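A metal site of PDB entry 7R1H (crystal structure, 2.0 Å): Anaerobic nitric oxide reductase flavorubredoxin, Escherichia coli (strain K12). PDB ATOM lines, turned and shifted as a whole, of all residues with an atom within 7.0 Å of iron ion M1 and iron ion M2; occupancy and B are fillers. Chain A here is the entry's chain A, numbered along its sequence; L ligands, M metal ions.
An oxygen (O2) of LG2 L2 is in hydrogen-bond range of the side-chain hydroxyl of Tyr 194 (3.3 Å).
A ring nitrogen (NE2) of His 147 sits close to an oxygen (O2) of LG2 L2 (3.4 Å).
A ring nitrogen (NE2) of His 23 lies within hydrogen-bond range of the side-chain carboxylate (OE2) of Glu 81, at 2.6 Å.
The side-chain hydroxyl (OG) of Ser 151 is in hydrogen-bond range of the backbone NH (N) of His 147.
ND1 of His 227 sits at hydrogen-bond distance from O of Ser 34 (2.8 Å).
N of Asp 166 lies within hydrogen-bond range of OG of Ser 226, 3.2 Å away.
OG of Ser 226 sits close to NE2 of His 84 (3.3 Å).
Four residues have an atom within 4 Å of iron ion M1: His 79, Glu 81, His 147 and Asp 166.
Of the 20 residues printed, 4 come within 4 Å of iron ion M2.
Along chain A the residues within 4 Å of iron ion M2 span positions 83 to 227.
Iron ion M1 is bound by OD2 of Asp 166 (2.0 Å), OE1 of Glu 81 (2.0 Å), O1 of LIG L1 (2.1 Å), NE2 of His 147 (2.2 Å) and NE2 of His 79 (2.4 Å).
Iron ion M1 has five donor atoms within binding distance.
Iron ion M2 is bound by O1 of LIG L1, NE2 of His 84, NE2 of His 227, OD1 of Asp 166 and OD2 of Asp 83.
Iron ion M2 has five donor atoms within binding distance.
Slightly farther from iron ion M2 lies O1 of LG2 L2 (2.7 Å).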
ATOM      1  N   PHE A  22      17.082   9.183  11.474  1.00  0.00           N
ATOM      2  CA  PHE A  22      16.433   9.129  10.164  1.00  0.00           C
ATOM      3  C   PHE A  22      17.073   8.030   9.324  1.00  0.00           C
ATOM      4  O   PHE A  22      18.271   7.767   9.452  1.00  0.00           O
ATOM      5  CB  PHE A  22      16.531  10.483   9.445  1.00  0.00           C
ATOM      6  CG  PHE A  22      15.245  11.260   9.438  1.00  0.00           C
ATOM      7  CD1 PHE A  22      14.885  12.022  10.540  1.00  0.00           C
ATOM      8  CD2 PHE A  22      14.416  11.245   8.337  1.00  0.00           C
ATOM      9  CE1 PHE A  22      13.695  12.743  10.540  1.00  0.00           C
ATOM     10  CE2 PHE A  22      13.230  11.963   8.328  1.00  0.00           C
ATOM     11  CZ  PHE A  22      12.872  12.716   9.435  1.00  0.00           C
ATOM     12  N   HIS A  23      16.284   7.390   8.465  1.00  0.00           N
ATOM     13  CA  HIS A  23      16.768   6.299   7.636  1.00  0.00           C
ATOM     14  C   HIS A  23      17.419   5.216   8.486  1.00  0.00           C
ATOM     15  O   HIS A  23      18.599   4.893   8.316  1.00  0.00           O
ATOM     16  CB  HIS A  23      17.760   6.819   6.590  1.00  0.00           C
ATOM     17  CG  HIS A  23      17.165   7.815   5.637  1.00  0.00           C
ATOM     18  ND1 HIS A  23      17.927   8.750   4.972  1.00  0.00           N
ATOM     19  CD2 HIS A  23      15.889   8.010   5.235  1.00  0.00           C
ATOM     20  CE1 HIS A  23      17.147   9.490   4.209  1.00  0.00           C
ATOM     21  NE2 HIS A  23      15.904   9.062   4.349  1.00  0.00           N
ATOM     22  N   SER A  34      11.605  18.869  11.284  1.00  0.00           N
ATOM     23  CA  SER A  34      10.226  19.282  11.050  1.00  0.00           C
ATOM     24  C   SER A  34       9.778  18.745   9.702  1.00  0.00           C
ATOM     25  O   SER A  34      10.594  18.497   8.817  1.00  0.00           O
ATOM     26  CB  SER A  34      10.090  20.802  11.106  1.00  0.00           C
ATOM     27  OG  SER A  34      10.846  21.415  10.082  1.00  0.00           O
ATOM     28  N   TYR A  35       8.470  18.540   9.557  1.00  0.00           N
ATOM     29  CA  TYR A  35       7.915  18.080   8.305  1.00  0.00           C
ATOM     30  C   TYR A  35       6.953  19.132   7.799  1.00  0.00           C
ATOM     31  O   TYR A  35       5.877  19.332   8.357  1.00  0.00           O
ATOM     32  CB  TYR A  35       7.230  16.717   8.481  1.00  0.00           C
ATOM     33  CG  TYR A  35       8.041  15.818   9.371  1.00  0.00           C
ATOM     34  CD1 TYR A  35       9.283  15.348   8.951  1.00  0.00           C
ATOM     35  CD2 TYR A  35       7.596  15.456  10.635  1.00  0.00           C
ATOM     36  CE1 TYR A  35      10.046  14.531   9.762  1.00  0.00           C
ATOM     37  CE2 TYR A  35       8.347  14.638  11.453  1.00  0.00           C
ATOM     38  CZ  TYR A  35       9.574  14.184  11.008  1.00  0.00           C
ATOM     39  OH  TYR A  35      10.337  13.368  11.820  1.00  0.00           O
ATOM     40  N   HIS A  79       7.411  14.381  -3.435  1.00  0.00           N
ATOM     41  CA  HIS A  79       8.366  13.365  -3.029  1.00  0.00           C
ATOM     42  C   HIS A  79       7.657  12.395  -2.105  1.00  0.00           C
ATOM     43  O   HIS A  79       7.024  12.810  -1.140  1.00  0.00           O
ATOM     44  CB  HIS A  79       9.569  14.036  -2.353  1.00  0.00           C
ATOM     45  CG  HIS A  79      10.621  13.083  -1.861  1.00  0.00           C
ATOM     46  ND1 HIS A  79      11.089  12.037  -2.623  1.00  0.00           N
ATOM     47  CD2 HIS A  79      11.305  13.043  -0.695  1.00  0.00           C
ATOM     48  CE1 HIS A  79      12.014  11.382  -1.937  1.00  0.00           C
ATOM     49  NE2 HIS A  79      12.160  11.978  -0.767  1.00  0.00           N
ATOM     50  N   ALA A  80       7.749  11.106  -2.404  1.00  0.00           N
ATOM     51  CA  ALA A  80       6.913  10.128  -1.719  1.00  0.00           C
ATOM     52  C   ALA A  80       7.649   9.373  -0.618  1.00  0.00           C
ATOM     53  O   ALA A  80       7.228   8.291  -0.222  1.00  0.00           O
ATOM     54  CB  ALA A  80       6.336   9.142  -2.726  1.00  0.00           C
ATOM     55  N   GLU A  81       8.737   9.937  -0.111  1.00  0.00           N
ATOM     56  CA  GLU A  81       9.407   9.320   1.020  1.00  0.00           C
ATOM     57  C   GLU A  81       8.484   9.460   2.230  1.00  0.00           C
ATOM     58  O   GLU A  81       7.732  10.424   2.331  1.00  0.00           O
ATOM     59  CB  GLU A  81      10.778   9.949   1.285  1.00  0.00           C
ATOM     60  CG  GLU A  81      11.628   9.140   2.259  1.00  0.00           C
ATOM     61  CD  GLU A  81      13.107   9.401   2.116  1.00  0.00           C
ATOM     62  OE1 GLU A  81      13.500  10.381   1.459  1.00  0.00           O
ATOM     63  OE2 GLU A  81      13.897   8.611   2.683  1.00  0.00           O
ATOM     64  N   GLU A  82       8.529   8.468   3.117  1.00  0.00           N
ATOM     65  CA  GLU A  82       7.552   8.344   4.203  1.00  0.00           C
ATOM     66  C   GLU A  82       7.412   9.568   5.092  1.00  0.00           C
ATOM     67  O   GLU A  82       6.358   9.776   5.691  1.00  0.00           O
ATOM     68  CB  GLU A  82       7.887   7.116   5.058  1.00  0.00           C
ATOM     69  CG  GLU A  82       8.002   7.391   6.557  1.00  0.00           C
ATOM     70  CD  GLU A  82       9.351   7.966   6.951  1.00  0.00           C
ATOM     71  OE1 GLU A  82      10.150   8.270   6.040  1.00  0.00           O
ATOM     72  OE2 GLU A  82       9.614   8.096   8.167  1.00  0.00           O
ATOM     73  N   ASP A  83       8.462  10.373   5.202  1.00  0.00           N
ATOM     74  CA  ASP A  83       8.416  11.529   6.078  1.00  0.00           C
ATOM     75  C   ASP A  83       7.626  12.688   5.474  1.00  0.00           C
ATOM     76  O   ASP A  83       7.374  13.689   6.139  1.00  0.00           O
ATOM     77  CB  ASP A  83       9.839  11.994   6.445  1.00  0.00           C
ATOM     78  CG  ASP A  83      10.698  12.243   5.232  1.00  0.00           C
ATOM     79  OD1 ASP A  83      10.425  11.619   4.183  1.00  0.00           O
ATOM     80  OD2 ASP A  83      11.650  13.047   5.323  1.00  0.00           O
ATOM     81  N   HIS A  84       7.233  12.540   4.209  1.00  0.00           N
ATOM     82  CA  HIS A  84       6.437  13.579   3.548  1.00  0.00           C
ATOM     83  C   HIS A  84       5.105  13.042   3.041  1.00  0.00           C
ATOM     84  O   HIS A  84       4.109  13.760   3.009  1.00  0.00           O
ATOM     85  CB  HIS A  84       7.227  14.202   2.395  1.00  0.00           C
ATOM     86  CG  HIS A  84       8.589  14.678   2.801  1.00  0.00           C
ATOM     87  ND1 HIS A  84       8.785  15.640   3.769  1.00  0.00           N
ATOM     88  CD2 HIS A  84       9.826  14.302   2.398  1.00  0.00           C
ATOM     89  CE1 HIS A  84      10.077  15.848   3.930  1.00  0.00           C
ATOM     90  NE2 HIS A  84      10.733  15.044   3.102  1.00  0.00           N
ATOM     91  N   HIS A 147      16.318  13.938  -4.327  1.00  0.00           N
ATOM     92  CA  HIS A 147      17.303  12.859  -4.384  1.00  0.00           C
ATOM     93  C   HIS A 147      16.714  11.506  -4.777  1.00  0.00           C
ATOM     94  O   HIS A 147      17.436  10.500  -4.803  1.00  0.00           O
ATOM     95  CB  HIS A 147      18.007  12.743  -3.026  1.00  0.00           C
ATOM     96  CG  HIS A 147      17.088  12.399  -1.893  1.00  0.00           C
ATOM     97  ND1 HIS A 147      16.967  11.122  -1.403  1.00  0.00           N
ATOM     98  CD2 HIS A 147      16.235  13.163  -1.170  1.00  0.00           C
ATOM     99  CE1 HIS A 147      16.081  11.109  -0.417  1.00  0.00           C
ATOM    100  NE2 HIS A 147      15.629  12.333  -0.260  1.00  0.00           N
ATOM    101  N   TRP A 148      15.424  11.463  -5.075  1.00  0.00           N
ATOM    102  CA  TRP A 148      14.775  10.232  -5.533  1.00  0.00           C
ATOM    103  C   TRP A 148      14.314  10.356  -6.976  1.00  0.00           C
ATOM    104  O   TRP A 148      14.240  11.456  -7.512  1.00  0.00           O
ATOM    105  CB  TRP A 148      13.569   9.885  -4.653  1.00  0.00           C
ATOM    106  CG  TRP A 148      13.885   9.016  -3.465  1.00  0.00           C
ATOM    107  CD1 TRP A 148      15.114   8.768  -2.933  1.00  0.00           C
ATOM    108  CD2 TRP A 148      12.951   8.307  -2.654  1.00  0.00           C
ATOM    109  NE1 TRP A 148      15.008   7.937  -1.840  1.00  0.00           N
ATOM    110  CE2 TRP A 148      13.676   7.637  -1.652  1.00  0.00           C
ATOM    111  CE3 TRP A 148      11.551   8.162  -2.678  1.00  0.00           C
ATOM    112  CZ2 TRP A 148      13.074   6.842  -0.685  1.00  0.00           C
ATOM    113  CZ3 TRP A 148      10.952   7.364  -1.719  1.00  0.00           C
ATOM    114  CH2 TRP A 148      11.707   6.709  -0.733  1.00  0.00           C
ATOM    115  N   SER A 151      11.275  12.725  -7.252  1.00  0.00           N
ATOM    116  CA  SER A 151      11.408  14.085  -6.732  1.00  0.00           C
ATOM    117  C   SER A 151      11.042  15.173  -7.741  1.00  0.00           C
ATOM    118  O   SER A 151      11.396  15.097  -8.921  1.00  0.00           O
ATOM    119  CB  SER A 151      12.840  14.329  -6.247  1.00  0.00           C
ATOM    120  OG  SER A 151      13.191  13.435  -5.209  1.00  0.00           O
ATOM    121  N   ASN A 165      10.608  20.861  -1.625  1.00  0.00           N
ATOM    122  CA  ASN A 165      10.683  19.618  -0.853  1.00  0.00           C
ATOM    123  C   ASN A 165      12.032  19.460  -0.143  1.00  0.00           C
ATOM    124  O   ASN A 165      12.483  20.386   0.532  1.00  0.00           O
ATOM    125  CB  ASN A 165      10.399  18.419  -1.750  1.00  0.00           C
ATOM    126  CG  ASN A 165      10.022  17.173  -0.952  1.00  0.00           C
ATOM    127  OD1 ASN A 165      10.865  16.304  -0.702  1.00  0.00           O
ATOM    128  ND2 ASN A 165       8.762  17.082  -0.540  1.00  0.00           N
ATOM    129  N   ASP A 166      12.682  18.321  -0.308  1.00  0.00           N
ATOM    130  CA  ASP A 166      13.917  18.021   0.423  1.00  0.00           C
ATOM    131  C   ASP A 166      15.050  19.013   0.130  1.00  0.00           C
ATOM    132  O   ASP A 166      15.816  19.372   1.025  1.00  0.00           O
ATOM    133  CB  ASP A 166      14.393  16.599   0.101  1.00  0.00           C
ATOM    134  CG  ASP A 166      13.762  15.556   0.996  1.00  0.00           C
ATOM    135  OD1 ASP A 166      13.235  15.925   2.061  1.00  0.00           O
ATOM    136  OD2 ASP A 166      13.782  14.364   0.637  1.00  0.00           O
ATOM    137  N   HIS A 171      17.488  19.405   8.776  1.00  0.00           N
ATOM    138  CA  HIS A 171      16.835  18.898   9.975  1.00  0.00           C
ATOM    139  C   HIS A 171      17.177  19.774  11.159  1.00  0.00           C
ATOM    140  O   HIS A 171      18.218  19.618  11.805  1.00  0.00           O
ATOM    141  CB  HIS A 171      17.222  17.430  10.217  1.00  0.00           C
ATOM    142  CG  HIS A 171      16.777  16.515   9.120  1.00  0.00           C
ATOM    143  ND1 HIS A 171      15.450  16.206   8.893  1.00  0.00           N
ATOM    144  CD2 HIS A 171      17.478  15.854   8.171  1.00  0.00           C
ATOM    145  CE1 HIS A 171      15.364  15.388   7.866  1.00  0.00           C
ATOM    146  NE2 HIS A 171      16.575  15.151   7.406  1.00  0.00           N
ATOM    147  N   TYR A 194      23.134  17.975   6.036  1.00  0.00           N
ATOM    148  CA  TYR A 194      22.175  17.318   5.157  1.00  0.00           C
ATOM    149  C   TYR A 194      22.754  17.074   3.771  1.00  0.00           C
ATOM    150  O   TYR A 194      22.668  15.959   3.241  1.00  0.00           O
ATOM    151  CB  TYR A 194      20.891  18.152   5.057  1.00  0.00           C
ATOM    152  CG  TYR A 194      19.822  17.462   4.238  1.00  0.00           C
ATOM    153  CD1 TYR A 194      19.626  17.787   2.897  1.00  0.00           C
ATOM    154  CD2 TYR A 194      19.030  16.476   4.794  1.00  0.00           C
ATOM    155  CE1 TYR A 194      18.652  17.149   2.144  1.00  0.00           C
ATOM    156  CE2 TYR A 194      18.056  15.833   4.054  1.00  0.00           C
ATOM    157  CZ  TYR A 194      17.870  16.174   2.735  1.00  0.00           C
ATOM    158  OH  TYR A 194      16.902  15.544   1.992  1.00  0.00           O
ATOM    159  N   ILE A 198      23.574  13.307   2.346  1.00  0.00           N
ATOM    160  CA  ILE A 198      22.452  12.885   1.497  1.00  0.00           C
ATOM    161  C   ILE A 198      22.656  13.184   0.014  1.00  0.00           C
ATOM    162  O   ILE A 198      22.447  12.327  -0.829  1.00  0.00           O
ATOM    163  CB  ILE A 198      21.143  13.563   1.941  1.00  0.00           C
ATOM    164  CG1 ILE A 198      20.826  13.205   3.399  1.00  0.00           C
ATOM    165  CG2 ILE A 198      19.991  13.162   1.023  1.00  0.00           C
ATOM    166  CD1 ILE A 198      20.650  11.733   3.655  1.00  0.00           C
ATOM    167  N   SER A 226      10.632  21.095   2.642  1.00  0.00           N
ATOM    168  CA  SER A 226       9.879  20.130   3.439  1.00  0.00           C
ATOM    169  C   SER A 226      10.525  19.859   4.801  1.00  0.00           C
ATOM    170  O   SER A 226       9.946  19.166   5.631  1.00  0.00           O
ATOM    171  CB  SER A 226       9.731  18.820   2.659  1.00  0.00           C
ATOM    172  OG  SER A 226      10.998  18.240   2.389  1.00  0.00           O
ATOM    173  N   HIS A 227      11.701  20.434   5.039  1.00  0.00           N
ATOM    174  CA  HIS A 227      12.386  20.295   6.328  1.00  0.00           C
ATOM    175  C   HIS A 227      12.962  21.607   6.826  1.00  0.00           C
ATOM    176  O   HIS A 227      13.769  22.243   6.142  1.00  0.00           O
ATOM    177  CB  HIS A 227      13.531  19.279   6.232  1.00  0.00           C
ATOM    178  CG  HIS A 227      13.087  17.865   6.056  1.00  0.00           C
ATOM    179  ND1 HIS A 227      12.354  17.195   7.008  1.00  0.00           N
ATOM    180  CD2 HIS A 227      13.282  16.984   5.048  1.00  0.00           C
ATOM    181  CE1 HIS A 227      12.107  15.964   6.596  1.00  0.00           C
ATOM    182  NE2 HIS A 227      12.663  15.815   5.406  1.00  0.00           N
HETATM  183  O1  LIG L   1      12.810  12.807   2.741  1.00  0.00           O
HETATM  184  O1  LG2 L   2      15.144  13.348   4.009  1.00  0.00           O
HETATM  185  O2  LG2 L   2      15.690  12.708   3.136  1.00  0.00           O
HETATM  186  N1  LG3 L   3      16.862   2.293  -4.171  1.00  0.00           N
HETATM  187  C1  LG3 L   3      17.564   1.792  -5.245  1.00  0.00           C
HETATM  188  O1  LG3 L   3      17.027   0.974  -5.990  1.00  0.00           O
HETATM  189  N2  LG3 L   3      18.865   2.190  -5.475  1.00  0.00           N
HETATM  190  C2  LG3 L   3      19.471   3.102  -4.634  1.00  0.00           C
HETATM  191  O2  LG3 L   3      20.624   3.466  -4.845  1.00  0.00           O
HETATM  192  C3  LG3 L   3      18.758   3.619  -3.548  1.00  0.00           C
HETATM  193  N3  LG3 L   3      19.351   4.530  -2.701  1.00  0.00           N
HETATM  194  C4  LG3 L   3      18.634   5.039  -1.626  1.00  0.00           C
HETATM  195  C5  LG3 L   3      19.231   5.958  -0.768  1.00  0.00           C
HETATM  196  C6  LG3 L   3      18.509   6.454   0.310  1.00  0.00           C
HETATM  197  C7  LG3 L   3      19.140   7.455   1.242  1.00  0.00           C
HETATM  198  C8  LG3 L   3      17.205   6.040   0.535  1.00  0.00           C
HETATM  199  C9  LG3 L   3      16.426   6.587   1.696  1.00  0.00           C
HETATM  200  C10 LG3 L   3      16.608   5.121  -0.323  1.00  0.00           C
HETATM  201  C11 LG3 L   3      17.326   4.616  -1.412  1.00  0.00           C
HETATM  202  N4  LG3 L   3      16.745   3.701  -2.252  1.00  0.00           N
HETATM  203  C12 LG3 L   3      17.455   3.204  -3.324  1.00  0.00           C
HETATM  204  C13 LG3 L   3      15.326   3.244  -2.025  1.00  0.00           C
HETATM  205  C14 LG3 L   3      15.241   2.192  -0.924  1.00  0.00           C
HETATM  206  O3  LG3 L   3      16.076   1.089  -1.235  1.00  0.00           O
HETATM  207  C15 LG3 L   3      13.798   1.739  -0.756  1.00  0.00           C
HETATM  208  O4  LG3 L   3      13.075   2.753  -0.068  1.00  0.00           O
HETATM  209  C16 LG3 L   3      13.683   0.419   0.011  1.00  0.00           C
HETATM  210  O5  LG3 L   3      12.406  -0.136  -0.231  1.00  0.00           O
HETATM  211  C17 LG3 L   3      13.852   0.632   1.514  1.00  0.00           C
HETATM  212  O6  LG3 L   3      14.123  -0.588   2.174  1.00  0.00           O
HETATM  213  P1  LG3 L   3      14.198  -0.594   3.784  1.00  0.00           P
HETATM  214  O7  LG3 L   3      14.257  -2.013   4.307  1.00  0.00           O
HETATM  215  O8  LG3 L   3      15.412   0.176   4.225  1.00  0.00           O
HETATM  216  O9  LG3 L   3      12.941   0.046   4.337  1.00  0.00           O
HETATM  217 FE    FE M   1      13.743  12.345   0.935  1.00  0.00          FE
HETATM  218 FE    FE M   2      12.672  14.498   3.716  1.00  0.00          FE
